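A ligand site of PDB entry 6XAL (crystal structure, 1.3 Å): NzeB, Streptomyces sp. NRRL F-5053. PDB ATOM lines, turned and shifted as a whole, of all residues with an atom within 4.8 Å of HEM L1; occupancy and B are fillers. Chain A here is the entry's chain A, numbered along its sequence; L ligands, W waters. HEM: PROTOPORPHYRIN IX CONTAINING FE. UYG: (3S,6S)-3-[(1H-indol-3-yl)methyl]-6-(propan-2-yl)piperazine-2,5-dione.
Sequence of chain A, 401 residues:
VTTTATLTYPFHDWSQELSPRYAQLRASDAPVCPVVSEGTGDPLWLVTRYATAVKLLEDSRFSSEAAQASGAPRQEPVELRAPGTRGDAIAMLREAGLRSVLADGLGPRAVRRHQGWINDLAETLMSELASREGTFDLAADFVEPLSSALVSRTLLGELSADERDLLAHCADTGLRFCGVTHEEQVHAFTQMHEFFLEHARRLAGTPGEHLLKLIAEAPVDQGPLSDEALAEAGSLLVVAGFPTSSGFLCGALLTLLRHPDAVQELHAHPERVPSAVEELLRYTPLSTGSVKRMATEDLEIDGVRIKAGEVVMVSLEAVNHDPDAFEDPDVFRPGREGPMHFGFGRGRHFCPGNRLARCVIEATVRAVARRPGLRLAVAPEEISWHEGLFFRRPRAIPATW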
ATOM      1  N   SER A  64      20.239  -8.642  13.005  1.00  0.00           N
ATOM      2  CA  SER A  64      19.793  -9.995  13.280  1.00  0.00           C
ATOM      3  C   SER A  64      20.973 -10.893  13.614  1.00  0.00           C
ATOM      4  O   SER A  64      20.950 -11.647  14.595  1.00  0.00           O
ATOM      5  CB  SER A  64      19.033 -10.552  12.075  1.00  0.00           C
ATOM      6  OG  SER A  64      18.741 -11.922  12.280  1.00  0.00           O
ATOM      7  N   GLN A  68      22.130 -13.439  16.902  1.00  0.00           N
ATOM      8  CA  GLN A  68      22.361 -14.861  16.738  1.00  0.00           C
ATOM      9  C   GLN A  68      23.682 -15.328  17.330  1.00  0.00           C
ATOM     10  O   GLN A  68      23.898 -16.544  17.441  1.00  0.00           O
ATOM     11  CB  GLN A  68      22.314 -15.260  15.252  1.00  0.00           C
ATOM     12  CG  GLN A  68      20.977 -15.035  14.524  1.00  0.00           C
ATOM     13  CD  GLN A  68      21.083 -15.198  13.014  1.00  0.00           C
ATOM     14  OE1 GLN A  68      21.713 -16.123  12.511  1.00  0.00           O
ATOM     15  NE2 GLN A  68      20.467 -14.275  12.274  1.00  0.00           N
ATOM     16  N   ILE A  90      24.285 -18.120   6.912  1.00  0.00           N
ATOM     17  CA  ILE A  90      24.082 -17.136   5.860  1.00  0.00           C
ATOM     18  C   ILE A  90      25.372 -16.345   5.595  1.00  0.00           C
ATOM     19  O   ILE A  90      25.710 -16.065   4.438  1.00  0.00           O
ATOM     20  CB  ILE A  90      22.871 -16.235   6.180  1.00  0.00           C
ATOM     21  CG1 ILE A  90      21.574 -17.034   6.071  1.00  0.00           C
ATOM     22  CG2 ILE A  90      22.855 -15.025   5.253  1.00  0.00           C
ATOM     23  CD1 ILE A  90      20.312 -16.258   6.425  1.00  0.00           C
ATOM     24  N   LEU A 102      20.219 -18.521  -1.632  1.00  0.00           N
ATOM     25  CA  LEU A 102      18.939 -18.963  -1.023  1.00  0.00           C
ATOM     26  C   LEU A 102      17.736 -18.328  -1.714  1.00  0.00           C
ATOM     27  O   LEU A 102      16.829 -19.035  -2.097  1.00  0.00           O
ATOM     28  CB  LEU A 102      18.929 -18.551   0.457  1.00  0.00           C
ATOM     29  CG  LEU A 102      20.019 -19.175   1.309  1.00  0.00           C
ATOM     30  CD1 LEU A 102      20.037 -18.545   2.694  1.00  0.00           C
ATOM     31  CD2 LEU A 102      19.810 -20.659   1.424  1.00  0.00           C
ATOM     32  N   LEU A 106      14.865 -20.239  -4.230  1.00  0.00           N
ATOM     33  CA  LEU A 106      13.534 -20.289  -3.639  1.00  0.00           C
ATOM     34  C   LEU A 106      12.577 -19.263  -4.236  1.00  0.00           C
ATOM     35  O   LEU A 106      11.439 -19.140  -3.753  1.00  0.00           O
ATOM     36  CB  LEU A 106      13.621 -20.097  -2.108  1.00  0.00           C
ATOM     37  CG  LEU A 106      14.456 -21.074  -1.285  1.00  0.00           C
ATOM     38  CD1 LEU A 106      14.783 -20.500   0.088  1.00  0.00           C
ATOM     39  CD2 LEU A 106      13.716 -22.385  -1.130  1.00  0.00           C
ATOM     40  N   LEU A 150       8.277 -31.572  -0.109  1.00  0.00           N
ATOM     41  CA  LEU A 150       8.841 -30.233  -0.271  1.00  0.00           C
ATOM     42  C   LEU A 150      10.308 -30.224   0.143  1.00  0.00           C
ATOM     43  O   LEU A 150      11.169 -29.684  -0.566  1.00  0.00           O
ATOM     44  CB  LEU A 150       8.047 -29.250   0.578  1.00  0.00           C
ATOM     45  CG  LEU A 150       8.335 -27.755   0.365  1.00  0.00           C
ATOM     46  CD1 LEU A 150       7.846 -27.350  -1.008  1.00  0.00           C
ATOM     47  CD2 LEU A 150       7.655 -26.928   1.446  1.00  0.00           C
ATOM     48  N   LEU A 155      14.763 -28.652  -1.059  1.00  0.00           N
ATOM     49  CA  LEU A 155      15.762 -28.209  -0.088  1.00  0.00           C
ATOM     50  C   LEU A 155      16.999 -29.104  -0.066  1.00  0.00           C
ATOM     51  O   LEU A 155      18.111 -28.617  -0.285  1.00  0.00           O
ATOM     52  CB  LEU A 155      15.152 -28.082   1.314  1.00  0.00           C
ATOM     53  CG  LEU A 155      14.002 -27.077   1.461  1.00  0.00           C
ATOM     54  CD1 LEU A 155      13.599 -26.854   2.912  1.00  0.00           C
ATOM     55  CD2 LEU A 155      14.348 -25.761   0.792  1.00  0.00           C
ATOM     56  N   LEU A 236      20.842 -25.305   8.315  1.00  0.00           N
ATOM     57  CA  LEU A 236      20.045 -24.100   8.112  1.00  0.00           C
ATOM     58  C   LEU A 236      18.733 -24.426   7.409  1.00  0.00           C
ATOM     59  O   LEU A 236      17.664 -23.952   7.813  1.00  0.00           O
ATOM     60  CB  LEU A 236      20.829 -23.064   7.315  1.00  0.00           C
ATOM     61  CG  LEU A 236      19.992 -21.972   6.612  1.00  0.00           C
ATOM     62  CD1 LEU A 236      19.443 -20.995   7.631  1.00  0.00           C
ATOM     63  CD2 LEU A 236      20.809 -21.241   5.570  1.00  0.00           C
ATOM     64  N   LEU A 237      18.798 -25.234   6.343  1.00  0.00           N
ATOM     65  CA  LEU A 237      17.610 -25.549   5.566  1.00  0.00           C
ATOM     66  C   LEU A 237      16.624 -26.379   6.377  1.00  0.00           C
ATOM     67  O   LEU A 237      15.408 -26.198   6.241  1.00  0.00           O
ATOM     68  CB  LEU A 237      18.012 -26.256   4.272  1.00  0.00           C
ATOM     69  CG  LEU A 237      18.802 -25.390   3.288  1.00  0.00           C
ATOM     70  CD1 LEU A 237      19.130 -26.156   2.027  1.00  0.00           C
ATOM     71  CD2 LEU A 237      18.017 -24.127   2.969  1.00  0.00           C
ATOM     72  N   ALA A 240      15.121 -23.863   9.130  1.00  0.00           N
ATOM     73  CA  ALA A 240      14.298 -22.788   8.585  1.00  0.00           C
ATOM     74  C   ALA A 240      13.116 -23.329   7.787  1.00  0.00           C
ATOM     75  O   ALA A 240      12.090 -22.636   7.670  1.00  0.00           O
ATOM     76  CB  ALA A 240      15.145 -21.898   7.668  1.00  0.00           C
ATOM     77  N   GLY A 241      13.235 -24.508   7.217  1.00  0.00           N
ATOM     78  CA  GLY A 241      12.270 -25.021   6.275  1.00  0.00           C
ATOM     79  C   GLY A 241      11.347 -26.135   6.754  1.00  0.00           C
ATOM     80  O   GLY A 241      10.219 -26.212   6.280  1.00  0.00           O
ATOM     81  N   THR A 244       8.684 -24.952  10.162  1.00  0.00           N
ATOM     82  CA  THR A 244       7.866 -23.816   9.724  1.00  0.00           C
ATOM     83  C   THR A 244       6.786 -24.293   8.760  1.00  0.00           C
ATOM     84  O   THR A 244       5.599 -24.034   8.968  1.00  0.00           O
ATOM     85  CB  THR A 244       8.798 -22.821   9.043  1.00  0.00           C
ATOM     86  OG1 THR A 244       9.602 -23.541   8.092  1.00  0.00           O
ATOM     87  CG2 THR A 244       9.681 -22.122  10.076  1.00  0.00           C
ATOM     88  N   SER A 245       7.180 -25.041   7.729  1.00  0.00           N
ATOM     89  CA  SER A 245       6.205 -25.519   6.752  1.00  0.00           C
ATOM     90  C   SER A 245       5.199 -26.464   7.397  1.00  0.00           C
ATOM     91  O   SER A 245       3.996 -26.348   7.144  1.00  0.00           O
ATOM     92  CB  SER A 245       6.932 -26.185   5.591  1.00  0.00           C
ATOM     93  OG  SER A 245       7.792 -25.259   4.951  1.00  0.00           O
ATOM     94  N   PHE A 248       2.993 -24.449   9.981  1.00  0.00           N
ATOM     95  CA  PHE A 248       2.081 -23.493   9.364  1.00  0.00           C
ATOM     96  C   PHE A 248       0.974 -24.196   8.593  1.00  0.00           C
ATOM     97  O   PHE A 248      -0.201 -23.796   8.677  1.00  0.00           O
ATOM     98  CB  PHE A 248       2.780 -22.462   8.481  1.00  0.00           C
ATOM     99  CG  PHE A 248       1.838 -21.391   8.041  1.00  0.00           C
ATOM    100  CD1 PHE A 248       1.574 -20.314   8.865  1.00  0.00           C
ATOM    101  CD2 PHE A 248       1.124 -21.508   6.862  1.00  0.00           C
ATOM    102  CE1 PHE A 248       0.648 -19.366   8.507  1.00  0.00           C
ATOM    103  CE2 PHE A 248       0.194 -20.558   6.494  1.00  0.00           C
ATOM    104  CZ  PHE A 248      -0.051 -19.496   7.318  1.00  0.00           C
ATOM    105  N   LEU A 281      -1.659 -16.131   6.447  1.00  0.00           N
ATOM    106  CA  LEU A 281      -0.335 -15.739   6.936  1.00  0.00           C
ATOM    107  C   LEU A 281      -0.431 -14.691   8.036  1.00  0.00           C
ATOM    108  O   LEU A 281       0.423 -14.652   8.920  1.00  0.00           O
ATOM    109  CB  LEU A 281       0.523 -15.262   5.765  1.00  0.00           C
ATOM    110  CG  LEU A 281       1.039 -16.408   4.886  1.00  0.00           C
ATOM    111  CD1 LEU A 281       1.397 -15.907   3.494  1.00  0.00           C
ATOM    112  CD2 LEU A 281       2.246 -17.073   5.548  1.00  0.00           C
ATOM    113  N   LEU A 286       2.217 -18.845  14.324  1.00  0.00           N
ATOM    114  CA  LEU A 286       3.244 -19.845  14.055  1.00  0.00           C
ATOM    115  C   LEU A 286       4.247 -19.941  15.193  1.00  0.00           C
ATOM    116  O   LEU A 286       4.148 -20.832  16.039  1.00  0.00           O
ATOM    117  CB  LEU A 286       3.909 -19.628  12.689  1.00  0.00           C
ATOM    118  CG  LEU A 286       4.915 -20.725  12.291  1.00  0.00           C
ATOM    119  CD1 LEU A 286       4.319 -22.149  12.319  1.00  0.00           C
ATOM    120  CD2 LEU A 286       5.510 -20.433  10.936  1.00  0.00           C
ATOM    121  N   VAL A 291      10.813 -12.778  16.572  1.00  0.00           N
ATOM    122  CA  VAL A 291      12.032 -12.426  15.841  1.00  0.00           C
ATOM    123  C   VAL A 291      12.793 -11.429  16.691  1.00  0.00           C
ATOM    124  O   VAL A 291      12.208 -10.715  17.514  1.00  0.00           O
ATOM    125  CB  VAL A 291      11.798 -11.887  14.414  1.00  0.00           C
ATOM    126  CG1 VAL A 291      10.873 -12.769  13.599  1.00  0.00           C
ATOM    127  CG2 VAL A 291      11.250 -10.559  14.434  1.00  0.00           C
ATOM    128  N   ARG A 293      16.549  -8.847  17.253  1.00  0.00           N
ATOM    129  CA  ARG A 293      17.631  -8.069  16.690  1.00  0.00           C
ATOM    130  C   ARG A 293      18.428  -7.453  17.833  1.00  0.00           C
ATOM    131  O   ARG A 293      17.876  -7.134  18.880  1.00  0.00           O
ATOM    132  CB  ARG A 293      17.116  -6.910  15.815  1.00  0.00           C
ATOM    133  CG  ARG A 293      16.182  -7.312  14.680  1.00  0.00           C
ATOM    134  CD  ARG A 293      16.923  -8.048  13.599  1.00  0.00           C
ATOM    135  NE  ARG A 293      16.091  -8.284  12.427  1.00  0.00           N
ATOM    136  CZ  ARG A 293      15.451  -9.429  12.182  1.00  0.00           C
ATOM    137  NH1 ARG A 293      15.531 -10.441  13.028  1.00  0.00           N
ATOM    138  NH2 ARG A 293      14.712  -9.538  11.092  1.00  0.00           N
ATOM    139  N   LEU A 316       5.578 -11.652  15.983  1.00  0.00           N
ATOM    140  CA  LEU A 316       4.868 -11.465  14.723  1.00  0.00           C
ATOM    141  C   LEU A 316       3.377 -11.675  14.935  1.00  0.00           C
ATOM    142  O   LEU A 316       2.549 -10.992  14.311  1.00  0.00           O
ATOM    143  CB  LEU A 316       5.402 -12.415  13.661  1.00  0.00           C
ATOM    144  CG  LEU A 316       6.907 -12.352  13.439  1.00  0.00           C
ATOM    145  CD1 LEU A 316       7.302 -13.311  12.347  1.00  0.00           C
ATOM    146  CD2 LEU A 316       7.335 -10.934  13.051  1.00  0.00           C
ATOM    147  N   PHE A 342       2.859  -9.511   8.795  1.00  0.00           N
ATOM    148  CA  PHE A 342       4.201  -9.812   9.297  1.00  0.00           C
ATOM    149  C   PHE A 342       4.505 -11.307   9.342  1.00  0.00           C
ATOM    150  O   PHE A 342       5.466 -11.713  10.002  1.00  0.00           O
ATOM    151  CB  PHE A 342       4.387  -9.209  10.693  1.00  0.00           C
ATOM    152  CG  PHE A 342       4.930  -7.788  10.720  1.00  0.00           C
ATOM    153  CD1 PHE A 342       4.188  -6.706  10.250  1.00  0.00           C
ATOM    154  CD2 PHE A 342       6.187  -7.529  11.258  1.00  0.00           C
ATOM    155  CE1 PHE A 342       4.694  -5.405  10.316  1.00  0.00           C
ATOM    156  CE2 PHE A 342       6.682  -6.236  11.328  1.00  0.00           C
ATOM    157  CZ  PHE A 342       5.936  -5.174  10.856  1.00  0.00           C
ATOM    158  N   GLY A 343       3.699 -12.145   8.672  1.00  0.00           N
ATOM    159  CA  GLY A 343       3.933 -13.578   8.758  1.00  0.00           C
ATOM    160  C   GLY A 343       5.285 -14.031   8.235  1.00  0.00           C
ATOM    161  O   GLY A 343       5.796 -15.082   8.678  1.00  0.00           O
ATOM    162  N   PHE A 344       5.862 -13.296   7.276  1.00  0.00           N
ATOM    163  CA  PHE A 344       7.191 -13.559   6.752  1.00  0.00           C
ATOM    164  C   PHE A 344       8.221 -12.561   7.266  1.00  0.00           C
ATOM    165  O   PHE A 344       9.339 -12.492   6.738  1.00  0.00           O
ATOM    166  CB  PHE A 344       7.173 -13.499   5.224  1.00  0.00           C
ATOM    167  CG  PHE A 344       6.456 -14.656   4.580  1.00  0.00           C
ATOM    168  CD1 PHE A 344       6.780 -15.982   4.867  1.00  0.00           C
ATOM    169  CD2 PHE A 344       5.492 -14.398   3.608  1.00  0.00           C
ATOM    170  CE1 PHE A 344       6.113 -17.036   4.219  1.00  0.00           C
ATOM    171  CE2 PHE A 344       4.842 -15.436   2.966  1.00  0.00           C
ATOM    172  CZ  PHE A 344       5.148 -16.758   3.262  1.00  0.00           C
ATOM    173  N   GLY A 345       7.861 -11.768   8.280  1.00  0.00           N
ATOM    174  CA  GLY A 345       8.763 -10.751   8.776  1.00  0.00           C
ATOM    175  C   GLY A 345       8.671  -9.472   7.948  1.00  0.00           C
ATOM    176  O   GLY A 345       7.640  -9.169   7.345  1.00  0.00           O
ATOM    177  N   HIS A 349      15.529  -9.171   6.297  1.00  0.00           N
ATOM    178  CA  HIS A 349      15.490 -10.590   6.560  1.00  0.00           C
ATOM    179  C   HIS A 349      14.149 -11.219   6.246  1.00  0.00           C
ATOM    180  O   HIS A 349      13.893 -12.349   6.676  1.00  0.00           O
ATOM    181  CB  HIS A 349      15.902 -10.872   8.010  1.00  0.00           C
ATOM    182  CG  HIS A 349      17.295 -10.406   8.305  1.00  0.00           C
ATOM    183  ND1 HIS A 349      18.392 -11.172   8.003  1.00  0.00           N
ATOM    184  CD2 HIS A 349      17.752  -9.257   8.851  1.00  0.00           C
ATOM    185  CE1 HIS A 349      19.486 -10.513   8.352  1.00  0.00           C
ATOM    186  NE2 HIS A 349      19.124  -9.348   8.858  1.00  0.00           N
ATOM    187  N   CYS A 351      11.409 -13.422   4.792  1.00  0.00           N
ATOM    188  CA  CYS A 351      11.620 -14.827   4.485  1.00  0.00           C
ATOM    189  C   CYS A 351      12.019 -15.027   3.017  1.00  0.00           C
ATOM    190  O   CYS A 351      11.217 -14.728   2.115  1.00  0.00           O
ATOM    191  CB  CYS A 351      10.329 -15.607   4.741  1.00  0.00           C
ATOM    192  SG  CYS A 351      10.491 -17.347   4.264  1.00  0.00           S
ATOM    193  N   PRO A 352      13.206 -15.569   2.749  1.00  0.00           N
ATOM    194  CA  PRO A 352      13.594 -15.833   1.353  1.00  0.00           C
ATOM    195  C   PRO A 352      12.863 -17.022   0.763  1.00  0.00           C
ATOM    196  O   PRO A 352      12.866 -17.177  -0.469  1.00  0.00           O
ATOM    197  CB  PRO A 352      15.100 -16.073   1.441  1.00  0.00           C
ATOM    198  CG  PRO A 352      15.316 -16.573   2.816  1.00  0.00           C
ATOM    199  CD  PRO A 352      14.297 -15.862   3.693  1.00  0.00           C
ATOM    200  N   GLY A 353      12.225 -17.826   1.594  1.00  0.00           N
ATOM    201  CA  GLY A 353      11.351 -18.882   1.123  1.00  0.00           C
ATOM    202  C   GLY A 353       9.917 -18.460   0.881  1.00  0.00           C
ATOM    203  O   GLY A 353       9.073 -19.324   0.620  1.00  0.00           O
ATOM    204  N   ALA A 357       6.773 -20.932   0.008  1.00  0.00           N
ATOM    205  CA  ALA A 357       5.784 -21.146   1.061  1.00  0.00           C
ATOM    206  C   ALA A 357       4.394 -20.745   0.587  1.00  0.00           C
ATOM    207  O   ALA A 357       3.441 -21.518   0.753  1.00  0.00           O
ATOM    208  CB  ALA A 357       6.190 -20.373   2.314  1.00  0.00           C
ATOM    209  N   ILE A 361       1.121 -23.251   0.458  1.00  0.00           N
ATOM    210  CA  ILE A 361      -0.101 -22.851   1.159  1.00  0.00           C
ATOM    211  C   ILE A 361      -1.261 -22.754   0.166  1.00  0.00           C
ATOM    212  O   ILE A 361      -2.355 -23.278   0.415  1.00  0.00           O
ATOM    213  CB  ILE A 361       0.101 -21.533   1.934  1.00  0.00           C
ATOM    214  CG1 ILE A 361       1.207 -21.675   2.997  1.00  0.00           C
ATOM    215  CG2 ILE A 361      -1.200 -21.156   2.620  1.00  0.00           C
ATOM    216  CD1 ILE A 361       1.812 -20.331   3.403  1.00  0.00           C
HETATM  217  CHA HEM L   1      13.256 -16.281   7.593  1.00  0.00           C
HETATM  218  CHB HEM L   1       8.521 -17.292   8.076  1.00  0.00           C
HETATM  219  CHC HEM L   1       9.098 -21.183   5.249  1.00  0.00           C
HETATM  220  CHD HEM L   1      13.807 -20.166   4.756  1.00  0.00           C
HETATM  221  C1A HEM L   1      11.935 -16.170   7.954  1.00  0.00           C
HETATM  222  C2A HEM L   1      11.352 -15.149   8.785  1.00  0.00           C
HETATM  223  C3A HEM L   1      10.053 -15.455   8.919  1.00  0.00           C
HETATM  224  C4A HEM L   1       9.754 -16.663   8.183  1.00  0.00           C
HETATM  225  CMA HEM L   1       9.007 -14.669   9.710  1.00  0.00           C
HETATM  226  CAA HEM L   1      12.070 -13.906   9.378  1.00  0.00           C
HETATM  227  CBA HEM L   1      12.835 -14.177  10.644  1.00  0.00           C
HETATM  228  CGA HEM L   1      13.515 -12.916  11.124  1.00  0.00           C
HETATM  229  O1A HEM L   1      13.129 -11.792  10.706  1.00  0.00           O
HETATM  230  O2A HEM L   1      14.461 -13.055  11.937  1.00  0.00           O
HETATM  231  C1B HEM L   1       8.249 -18.437   7.373  1.00  0.00           C
HETATM  232  C2B HEM L   1       6.959 -19.080   7.223  1.00  0.00           C
HETATM  233  C3B HEM L   1       7.135 -20.173   6.456  1.00  0.00           C
HETATM  234  C4B HEM L   1       8.533 -20.227   6.072  1.00  0.00           C
HETATM  235  CMB HEM L   1       5.663 -18.559   7.888  1.00  0.00           C
HETATM  236  CAB HEM L   1       6.091 -21.211   5.974  1.00  0.00           C
HETATM  237  CBB HEM L   1       4.767 -21.021   6.008  1.00  0.00           C
HETATM  238  C1C HEM L   1      10.419 -21.239   4.843  1.00  0.00           C
HETATM  239  C2C HEM L   1      10.985 -22.276   4.005  1.00  0.00           C
HETATM  240  C3C HEM L   1      12.296 -21.995   3.884  1.00  0.00           C
HETATM  241  C4C HEM L   1      12.584 -20.795   4.623  1.00  0.00           C
HETATM  242  CMC HEM L   1      10.206 -23.463   3.382  1.00  0.00           C
HETATM  243  CAC HEM L   1      13.296 -22.829   3.060  1.00  0.00           C
HETATM  244  CBC HEM L   1      14.535 -23.042   3.523  1.00  0.00           C
HETATM  245  C1D HEM L   1      14.083 -19.079   5.535  1.00  0.00           C
HETATM  246  C2D HEM L   1      15.395 -18.557   5.854  1.00  0.00           C
HETATM  247  C3D HEM L   1      15.253 -17.494   6.633  1.00  0.00           C
HETATM  248  C4D HEM L   1      13.828 -17.297   6.856  1.00  0.00           C
HETATM  249  CMD HEM L   1      16.710 -19.178   5.339  1.00  0.00           C
HETATM  250  CAD HEM L   1      16.401 -16.632   7.238  1.00  0.00           C
HETATM  251  CBD HEM L   1      16.533 -15.298   6.533  1.00  0.00           C
HETATM  252  CGD HEM L   1      17.414 -14.353   7.323  1.00  0.00           C
HETATM  253  O1D HEM L   1      17.582 -14.524   8.567  1.00  0.00           O
HETATM  254  O2D HEM L   1      17.938 -13.436   6.662  1.00  0.00           O
HETATM  255  NA  HEM L   1      10.943 -17.077   7.605  1.00  0.00           N
HETATM  256  NB  HEM L   1       9.206 -19.137   6.647  1.00  0.00           N
HETATM  257  NC  HEM L   1      11.413 -20.344   5.200  1.00  0.00           N
HETATM  258  ND  HEM L   1      13.127 -18.281   6.180  1.00  0.00           N
HETATM  259 FE   HEM L   1      11.099 -18.572   6.180  1.00  0.00          FE
HETATM  260  C10 UYG L   2      14.124 -20.979  12.447  1.00  0.00           C
HETATM  261  C11 UYG L   2      19.544 -18.619  11.243  1.00  0.00           C
HETATM  262  C12 UYG L   2      19.159 -20.071  10.943  1.00  0.00           C
HETATM  263  C13 UYG L   2      17.651 -20.232  10.741  1.00  0.00           C
HETATM  264  N   UYG L   2      14.276 -19.053  10.746  1.00  0.00           N
HETATM  265  C   UYG L   2      18.316 -17.253  13.056  1.00  0.00           C
HETATM  266  O   UYG L   2      18.109 -17.059  14.218  1.00  0.00           O
HETATM  267  C1  UYG L   2      17.613 -16.369  12.026  1.00  0.00           C
HETATM  268  C14 UYG L   2      19.608 -20.962  12.104  1.00  0.00           C
HETATM  269  C15 UYG L   2      18.951 -17.627  10.240  1.00  0.00           C
HETATM  270  C2  UYG L   2      16.081 -16.443  12.192  1.00  0.00           C
HETATM  271  C3  UYG L   2      15.355 -17.765  11.831  1.00  0.00           C
HETATM  272  C4  UYG L   2      14.777 -17.883  10.680  1.00  0.00           C
HETATM  273  C5  UYG L   2      14.466 -19.746  11.921  1.00  0.00           C
HETATM  274  C6  UYG L   2      15.237 -18.798  12.715  1.00  0.00           C
HETATM  275  C7  UYG L   2      15.623 -19.142  13.988  1.00  0.00           C
HETATM  276  C8  UYG L   2      15.278 -20.394  14.513  1.00  0.00           C
HETATM  277  C9  UYG L   2      14.523 -21.306  13.741  1.00  0.00           C
HETATM  278  N1  UYG L   2      18.019 -16.588  10.652  1.00  0.00           N
HETATM  279  N2  UYG L   2      19.203 -18.312  12.627  1.00  0.00           N
HETATM  280  O1  UYG L   2      19.225 -17.724   9.088  1.00  0.00           O
HETATM  281  C10 UYG L   3       8.351 -17.738  11.771  1.00  0.00           C
HETATM  282  C11 UYG L   3      13.161 -18.969  17.417  1.00  0.00           C
HETATM  283  C12 UYG L   3      12.768 -18.885  18.895  1.00  0.00           C
HETATM  284  C13 UYG L   3      14.008 -18.858  19.797  1.00  0.00           C
HETATM  285  N   UYG L   3       8.578 -16.194  13.834  1.00  0.00           N
HETATM  286  C   UYG L   3      13.871 -17.023  15.875  1.00  0.00           C
HETATM  287  O   UYG L   3      14.669 -16.171  15.657  1.00  0.00           O
HETATM  288  C1  UYG L   3      12.680 -17.231  14.930  1.00  0.00           C
HETATM  289  C14 UYG L   3      11.914 -17.642  19.132  1.00  0.00           C
HETATM  290  C15 UYG L   3      11.842 -18.959  16.644  1.00  0.00           C
HETATM  291  C2  UYG L   3      12.003 -15.902  14.531  1.00  0.00           C
HETATM  292  C3  UYG L   3      10.572 -16.185  13.986  1.00  0.00           C
HETATM  293  C4  UYG L   3       9.510 -15.696  14.567  1.00  0.00           C
HETATM  294  C5  UYG L   3       8.940 -17.005  12.782  1.00  0.00           C
HETATM  295  C6  UYG L   3      10.400 -16.990  12.891  1.00  0.00           C
HETATM  296  C7  UYG L   3      11.161 -17.716  11.991  1.00  0.00           C
HETATM  297  C8  UYG L   3      10.553 -18.453  10.965  1.00  0.00           C
HETATM  298  C9  UYG L   3       9.137 -18.469  10.881  1.00  0.00           C
HETATM  299  N1  UYG L   3      11.669 -18.126  15.475  1.00  0.00           N
HETATM  300  N2  UYG L   3      14.055 -17.868  17.048  1.00  0.00           N
HETATM  301  O1  UYG L   3      10.932 -19.654  16.993  1.00  0.00           O
HETATM  302  O   HOH W   1      12.103 -10.316   8.707  1.00  0.00           O
HETATM  303  O   HOH W   2      20.249 -13.928   9.415  1.00  0.00           O
HETATM  304  O   HOH W   3      16.963 -12.857  10.732  1.00  0.00           O
HETATM  305  O   HOH W   4      17.904 -13.295   4.084  1.00  0.00           O
HETATM  306  O   HOH W   5      14.857 -13.614  14.537  1.00  0.00           O
HETATM  307  O   HOH W   6      12.404 -20.035   8.535  1.00  0.00           O
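O of Ala 240 lies close to NC of HEM L1, at 3.4 Å.
Residues that only touch HEM L1: Ile 90 (3.6 Å), Leu 155 (3.9 Å), Leu 237 (3.7 Å), Gly 241 (3.8 Å), Thr 244 (3.7 Å), Ser 245 (3.4 Å), Phe 248 (3.5 Å), Leu 286 (3.6 Å), Val 291 (3.6 Å), Leu 316 (3.4 Å), Gly 343 (3.4 Å), Phe 344 (3.3 Å), Gly 345 (3.4 Å), Pro 352 (3.5 Å), Ala 357 (3.8 Å) and Ile 361 (3.999 Å).
Hydrophobic or aromatic side chains that line HEM L1: Ile 90, Leu 155, Leu 237, Ala 240, Phe 248, Leu 286, Val 291, Leu 316, Phe 344, His 349, Pro 352, Ala 357 and Ile 361.
Within 4 Å of HEM L1: Ile 90, Leu 155, Leu 237, Ala 240, Gly 241, Thr 244, Ser 245, Phe 248, Leu 286, Val 291, Arg 293, Leu 316, Gly 343, Phe 344, Gly 345, His 349, Cys 351, Pro 352, Ala 357 and Ile 361.
Along chain A the residues within 4 Å of HEM L1 span positions 90 to 361.
A nitrogen (N1) of UYG L2 is in hydrogen-bond range of an oxygen (O1D) of HEM L1 (3.0 Å).
Water W1 bridges O1A of HEM L1 and O of His 349.
Water W5 bridges an oxygen (O2A) of HEM L1 and an oxygen (O) of UYG L3.
Water W3 lies within hydrogen-bond range of OG of Ser 64 (2.5 Å) and O2A of HEM L1 (2.8 Å).
Water W2 bridges an oxygen (O1D) of HEM L1 (2.9 Å) and the side-chain amide nitrogen (NE2) of Gln 68 (2.9 Å).
Water W6 lies within hydrogen-bond range of the backbone carbonyl oxygen (O) of Ala 240 and a nitrogen (N) of UYG L2.
SG of Cys 351 sits close to N of Gly 353.
The side-chain hydroxyl (OG1) of Thr 244 sits at hydrogen-bond distance from the backbone carbonyl oxygen (O) of Gly 241 (3.3 Å).
N of Cys 351 is in hydrogen-bond range of O of Phe 344 (3.0 Å).
O of Gly 241 sits at hydrogen-bond distance from OG of Ser 245, 2.9 Å away.
The backbone carbonyl oxygen of Ala 240 sits at hydrogen-bond distance from the side-chain hydroxyl of Thr 244.
The side-chain sulfur (SG) of Cys 351 is bound to an iron atom (FE) of HEM L1.
O2D of HEM L1 sits at hydrogen-bond distance from ND1 of His 349 (2.7 Å).
N2 of UYG L2 is in hydrogen-bond range of OE1 of Gln 68, 3.3 Å away.
The guanidinium group (NH2) of Arg 293 is in salt-bridge range of an oxygen (O1A) of HEM L1, 2.8 Å away.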
